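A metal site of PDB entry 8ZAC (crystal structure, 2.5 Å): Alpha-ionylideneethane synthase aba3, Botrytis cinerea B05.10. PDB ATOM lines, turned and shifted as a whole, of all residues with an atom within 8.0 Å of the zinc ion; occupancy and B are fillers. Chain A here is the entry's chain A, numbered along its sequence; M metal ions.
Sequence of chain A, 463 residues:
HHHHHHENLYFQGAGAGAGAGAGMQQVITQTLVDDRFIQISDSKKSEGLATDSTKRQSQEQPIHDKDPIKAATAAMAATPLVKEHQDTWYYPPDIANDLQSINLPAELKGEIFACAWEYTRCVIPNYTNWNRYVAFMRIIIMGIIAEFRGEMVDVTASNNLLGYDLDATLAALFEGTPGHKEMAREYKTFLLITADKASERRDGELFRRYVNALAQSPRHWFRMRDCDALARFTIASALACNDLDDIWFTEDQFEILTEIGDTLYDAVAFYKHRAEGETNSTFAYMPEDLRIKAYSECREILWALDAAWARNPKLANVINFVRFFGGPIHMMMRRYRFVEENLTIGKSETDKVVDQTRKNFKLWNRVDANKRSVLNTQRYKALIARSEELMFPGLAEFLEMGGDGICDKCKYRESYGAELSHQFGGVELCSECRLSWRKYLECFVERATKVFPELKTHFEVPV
The backbone NH (N) of Glu 432 sits close to the side-chain sulfur (SG) of Cys 430, at 3.7 Å.
OG of Ser 436 is in hydrogen-bond range of O of Cys 433, at 3.1 Å.
The side-chain hydroxyl (OH) of Tyr 412 is in hydrogen-bond range of the backbone carbonyl oxygen (O) of Cys 407, at 3.1 Å.
SG of Cys 407 binds the zinc ion (2.3 Å).
SG of Cys 410 is bound to the zinc ion, at 2.3 Å.
SG of Cys 433 is bound to the zinc ion (2.3 Å).
The zinc ion is bound by SG of Cys 430 (2.4 Å).
Of the 19 residues printed, 4 come within 4 Å of the zinc ion.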
ATOM      1  N   ALA A 215       1.636 -15.080 -14.233  1.00  0.00           N
ATOM      2  CA  ALA A 215       1.298 -15.369 -12.820  1.00  0.00           C
ATOM      3  C   ALA A 215       1.189 -14.078 -12.006  1.00  0.00           C
ATOM      4  O   ALA A 215       1.227 -14.175 -10.766  1.00  0.00           O
ATOM      5  CB  ALA A 215       2.339 -16.308 -12.248  1.00  0.00           C
ATOM      6  N   GLN A 216       1.077 -12.928 -12.661  1.00  0.00           N
ATOM      7  CA  GLN A 216       0.966 -11.616 -11.965  1.00  0.00           C
ATOM      8  C   GLN A 216      -0.435 -11.509 -11.359  1.00  0.00           C
ATOM      9  O   GLN A 216      -0.583 -11.014 -10.223  1.00  0.00           O
ATOM     10  CB  GLN A 216       1.369 -10.448 -12.886  1.00  0.00           C
ATOM     11  CG  GLN A 216       0.419 -10.113 -14.028  1.00  0.00           C
ATOM     12  CD  GLN A 216       1.040  -9.100 -14.973  1.00  0.00           C
ATOM     13  OE1 GLN A 216       0.887  -9.155 -16.203  1.00  0.00           O
ATOM     14  NE2 GLN A 216       1.771  -8.149 -14.416  1.00  0.00           N
ATOM     15  N   ILE A 406       6.027  -9.179  -9.585  1.00  0.00           N
ATOM     16  CA  ILE A 406       5.571  -8.110  -8.652  1.00  0.00           C
ATOM     17  C   ILE A 406       5.733  -8.644  -7.218  1.00  0.00           C
ATOM     18  O   ILE A 406       6.318  -7.937  -6.350  1.00  0.00           O
ATOM     19  CB  ILE A 406       4.144  -7.653  -9.015  1.00  0.00           C
ATOM     20  CG1 ILE A 406       4.133  -6.871 -10.337  1.00  0.00           C
ATOM     21  CG2 ILE A 406       3.495  -6.856  -7.885  1.00  0.00           C
ATOM     22  CD1 ILE A 406       2.757  -6.683 -10.941  1.00  0.00           C
ATOM     23  N   CYS A 407       5.324  -9.878  -6.993  1.00  0.00           N
ATOM     24  CA  CYS A 407       5.206 -10.482  -5.644  1.00  0.00           C
ATOM     25  C   CYS A 407       6.576 -10.991  -5.152  1.00  0.00           C
ATOM     26  O   CYS A 407       7.471 -11.213  -5.984  1.00  0.00           O
ATOM     27  CB  CYS A 407       4.185 -11.598  -5.679  1.00  0.00           C
ATOM     28  SG  CYS A 407       3.705 -12.123  -4.017  1.00  0.00           S
ATOM     29  N   ASP A 408       6.724 -11.132  -3.829  1.00  0.00           N
ATOM     30  CA  ASP A 408       8.018 -11.441  -3.164  1.00  0.00           C
ATOM     31  C   ASP A 408       7.924 -12.723  -2.335  1.00  0.00           C
ATOM     32  O   ASP A 408       8.972 -13.391  -2.187  1.00  0.00           O
ATOM     33  CB  ASP A 408       8.503 -10.248  -2.350  1.00  0.00           C
ATOM     34  CG  ASP A 408       9.144  -9.160  -3.200  1.00  0.00           C
ATOM     35  OD1 ASP A 408      10.029  -9.505  -4.017  1.00  0.00           O
ATOM     36  OD2 ASP A 408       8.749  -7.992  -3.037  1.00  0.00           O
ATOM     37  N   LYS A 409       6.741 -13.099  -1.833  1.00  0.00           N
ATOM     38  CA  LYS A 409       6.547 -14.440  -1.214  1.00  0.00           C
ATOM     39  C   LYS A 409       6.392 -15.485  -2.339  1.00  0.00           C
ATOM     40  O   LYS A 409       6.609 -16.689  -2.059  1.00  0.00           O
ATOM     41  CB  LYS A 409       5.369 -14.403  -0.231  1.00  0.00           C
ATOM     42  CG  LYS A 409       5.384 -15.492   0.843  1.00  0.00           C
ATOM     43  CD  LYS A 409       6.486 -15.330   1.878  1.00  0.00           C
ATOM     44  CE  LYS A 409       6.283 -16.196   3.108  1.00  0.00           C
ATOM     45  NZ  LYS A 409       7.024 -15.667   4.287  1.00  0.00           N
ATOM     46  N   CYS A 410       6.061 -15.056  -3.562  1.00  0.00           N
ATOM     47  CA  CYS A 410       5.984 -15.901  -4.791  1.00  0.00           C
ATOM     48  C   CYS A 410       7.378 -16.370  -5.223  1.00  0.00           C
ATOM     49  O   CYS A 410       8.302 -15.552  -5.182  1.00  0.00           O
ATOM     50  CB  CYS A 410       5.344 -15.127  -5.951  1.00  0.00           C
ATOM     51  SG  CYS A 410       3.548 -15.353  -6.052  1.00  0.00           S
ATOM     52  N   LYS A 411       7.502 -17.636  -5.655  1.00  0.00           N
ATOM     53  CA  LYS A 411       8.790 -18.288  -6.002  1.00  0.00           C
ATOM     54  C   LYS A 411       8.921 -18.359  -7.531  1.00  0.00           C
ATOM     55  O   LYS A 411       8.188 -19.130  -8.165  1.00  0.00           O
ATOM     56  CB  LYS A 411       8.867 -19.670  -5.330  1.00  0.00           C
ATOM     57  CG  LYS A 411       8.809 -19.657  -3.802  1.00  0.00           C
ATOM     58  CD  LYS A 411      10.112 -19.258  -3.124  1.00  0.00           C
ATOM     59  CE  LYS A 411      10.017 -19.161  -1.618  1.00  0.00           C
ATOM     60  NZ  LYS A 411      11.358 -19.255  -0.977  1.00  0.00           N
ATOM     61  N   TYR A 412       9.850 -17.582  -8.085  1.00  0.00           N
ATOM     62  CA  TYR A 412      10.181 -17.502  -9.535  1.00  0.00           C
ATOM     63  C   TYR A 412      11.355 -18.444  -9.806  1.00  0.00           C
ATOM     64  O   TYR A 412      11.666 -19.265  -8.924  1.00  0.00           O
ATOM     65  CB  TYR A 412      10.471 -16.056  -9.941  1.00  0.00           C
ATOM     66  CG  TYR A 412       9.358 -15.098  -9.589  1.00  0.00           C
ATOM     67  CD1 TYR A 412       9.187 -14.637  -8.285  1.00  0.00           C
ATOM     68  CD2 TYR A 412       8.429 -14.679 -10.541  1.00  0.00           C
ATOM     69  CE1 TYR A 412       8.158 -13.785  -7.943  1.00  0.00           C
ATOM     70  CE2 TYR A 412       7.397 -13.817 -10.209  1.00  0.00           C
ATOM     71  CZ  TYR A 412       7.261 -13.368  -8.903  1.00  0.00           C
ATOM     72  OH  TYR A 412       6.263 -12.524  -8.546  1.00  0.00           O
ATOM     73  N   VAL A 427       5.846 -19.979 -12.328  1.00  0.00           N
ATOM     74  CA  VAL A 427       5.857 -19.326 -10.980  1.00  0.00           C
ATOM     75  C   VAL A 427       5.046 -20.207 -10.029  1.00  0.00           C
ATOM     76  O   VAL A 427       3.970 -20.655 -10.438  1.00  0.00           O
ATOM     77  CB  VAL A 427       5.301 -17.891 -11.004  1.00  0.00           C
ATOM     78  CG1 VAL A 427       5.270 -17.289  -9.607  1.00  0.00           C
ATOM     79  CG2 VAL A 427       6.051 -16.969 -11.963  1.00  0.00           C
ATOM     80  N   GLU A 428       5.536 -20.432  -8.807  1.00  0.00           N
ATOM     81  CA  GLU A 428       4.766 -21.108  -7.723  1.00  0.00           C
ATOM     82  C   GLU A 428       4.190 -20.023  -6.808  1.00  0.00           C
ATOM     83  O   GLU A 428       4.946 -19.416  -6.039  1.00  0.00           O
ATOM     84  CB  GLU A 428       5.649 -22.134  -6.995  1.00  0.00           C
ATOM     85  CG  GLU A 428       4.893 -22.980  -5.983  1.00  0.00           C
ATOM     86  CD  GLU A 428       5.803 -23.685  -4.991  1.00  0.00           C
ATOM     87  OE1 GLU A 428       6.342 -24.769  -5.349  1.00  0.00           O
ATOM     88  OE2 GLU A 428       6.012 -23.135  -3.878  1.00  0.00           O
ATOM     89  N   LEU A 429       2.896 -19.768  -6.918  1.00  0.00           N
ATOM     90  CA  LEU A 429       2.211 -18.663  -6.207  1.00  0.00           C
ATOM     91  C   LEU A 429       2.285 -18.915  -4.698  1.00  0.00           C
ATOM     92  O   LEU A 429       2.397 -20.080  -4.291  1.00  0.00           O
ATOM     93  CB  LEU A 429       0.758 -18.567  -6.705  1.00  0.00           C
ATOM     94  CG  LEU A 429       0.565 -18.191  -8.171  1.00  0.00           C
ATOM     95  CD1 LEU A 429      -0.912 -18.260  -8.564  1.00  0.00           C
ATOM     96  CD2 LEU A 429       1.093 -16.809  -8.479  1.00  0.00           C
ATOM     97  N   CYS A 430       2.214 -17.845  -3.902  1.00  0.00           N
ATOM     98  CA  CYS A 430       2.269 -17.827  -2.422  1.00  0.00           C
ATOM     99  C   CYS A 430       0.866 -17.976  -1.811  1.00  0.00           C
ATOM    100  O   CYS A 430      -0.136 -17.792  -2.545  1.00  0.00           O
ATOM    101  CB  CYS A 430       2.853 -16.503  -1.927  1.00  0.00           C
ATOM    102  SG  CYS A 430       1.824 -15.082  -2.375  1.00  0.00           S
ATOM    103  N   SER A 431       0.822 -18.271  -0.513  1.00  0.00           N
ATOM    104  CA  SER A 431      -0.415 -18.428   0.301  1.00  0.00           C
ATOM    105  C   SER A 431      -1.439 -17.345  -0.052  1.00  0.00           C
ATOM    106  O   SER A 431      -2.651 -17.697  -0.147  1.00  0.00           O
ATOM    107  CB  SER A 431      -0.069 -18.424   1.787  1.00  0.00           C
ATOM    108  OG  SER A 431      -1.159 -17.969   2.583  1.00  0.00           O
ATOM    109  N   GLU A 432      -0.994 -16.096  -0.193  1.00  0.00           N
ATOM    110  CA  GLU A 432      -1.869 -14.897  -0.341  1.00  0.00           C
ATOM    111  C   GLU A 432      -2.359 -14.750  -1.803  1.00  0.00           C
ATOM    112  O   GLU A 432      -3.535 -14.401  -1.996  1.00  0.00           O
ATOM    113  CB  GLU A 432      -1.130 -13.617   0.090  1.00  0.00           C
ATOM    114  CG  GLU A 432      -2.032 -12.408   0.171  1.00  0.00           C
ATOM    115  CD  GLU A 432      -1.358 -11.055   0.030  1.00  0.00           C
ATOM    116  OE1 GLU A 432      -0.214 -10.908   0.506  1.00  0.00           O
ATOM    117  OE2 GLU A 432      -1.993 -10.140  -0.550  1.00  0.00           O
ATOM    118  N   CYS A 433      -1.468 -14.935  -2.786  1.00  0.00           N
ATOM    119  CA  CYS A 433      -1.795 -14.842  -4.233  1.00  0.00           C
ATOM    120  C   CYS A 433      -2.738 -16.004  -4.591  1.00  0.00           C
ATOM    121  O   CYS A 433      -3.805 -15.745  -5.164  1.00  0.00           O
ATOM    122  CB  CYS A 433      -0.532 -14.842  -5.091  1.00  0.00           C
ATOM    123  SG  CYS A 433       0.424 -13.285  -5.062  1.00  0.00           S
ATOM    124  N   ARG A 434      -2.406 -17.232  -4.172  1.00  0.00           N
ATOM    125  CA  ARG A 434      -3.248 -18.452  -4.311  1.00  0.00           C
ATOM    126  C   ARG A 434      -4.675 -18.183  -3.803  1.00  0.00           C
ATOM    127  O   ARG A 434      -5.608 -18.796  -4.366  1.00  0.00           O
ATOM    128  CB  ARG A 434      -2.651 -19.641  -3.549  1.00  0.00           C
ATOM    129  CG  ARG A 434      -1.625 -20.460  -4.338  1.00  0.00           C
ATOM    130  CD  ARG A 434      -0.893 -21.502  -3.515  1.00  0.00           C
ATOM    131  NE  ARG A 434      -1.778 -22.163  -2.559  1.00  0.00           N
ATOM    132  CZ  ARG A 434      -1.386 -22.795  -1.451  1.00  0.00           C
ATOM    133  NH1 ARG A 434      -0.100 -22.867  -1.130  1.00  0.00           N
ATOM    134  NH2 ARG A 434      -2.298 -23.339  -0.663  1.00  0.00           N
ATOM    135  N   SER A 436      -6.247 -14.981  -3.635  1.00  0.00           N
ATOM    136  CA  SER A 436      -6.871 -13.927  -4.478  1.00  0.00           C
ATOM    137  C   SER A 436      -7.293 -14.537  -5.837  1.00  0.00           C
ATOM    138  O   SER A 436      -8.390 -14.203  -6.354  1.00  0.00           O
ATOM    139  CB  SER A 436      -5.974 -12.724  -4.658  1.00  0.00           C
ATOM    140  OG  SER A 436      -5.041 -12.938  -5.715  1.00  0.00           O
ATOM    141  N   TRP A 437      -6.451 -15.434  -6.358  1.00  0.00           N
ATOM    142  CA  TRP A 437      -6.751 -16.306  -7.517  1.00  0.00           C
ATOM    143  C   TRP A 437      -7.962 -17.185  -7.166  1.00  0.00           C
ATOM    144  O   TRP A 437      -8.940 -17.202  -7.956  1.00  0.00           O
ATOM    145  CB  TRP A 437      -5.531 -17.141  -7.873  1.00  0.00           C
ATOM    146  CG  TRP A 437      -4.450 -16.323  -8.499  1.00  0.00           C
ATOM    147  CD1 TRP A 437      -3.801 -15.250  -7.958  1.00  0.00           C
ATOM    148  CD2 TRP A 437      -3.878 -16.503  -9.801  1.00  0.00           C
ATOM    149  NE1 TRP A 437      -2.853 -14.776  -8.817  1.00  0.00           N
ATOM    150  CE2 TRP A 437      -2.883 -15.524  -9.966  1.00  0.00           C
ATOM    151  CE3 TRP A 437      -4.110 -17.409 -10.850  1.00  0.00           C
ATOM    152  CZ2 TRP A 437      -2.115 -15.419 -11.112  1.00  0.00           C
ATOM    153  CZ3 TRP A 437      -3.341 -17.304 -11.996  1.00  0.00           C
ATOM    154  CH2 TRP A 437      -2.371 -16.320 -12.122  1.00  0.00           C
HETATM  155 ZN    ZN M   1       2.522 -14.076  -4.387  1.00  0.00          ZN
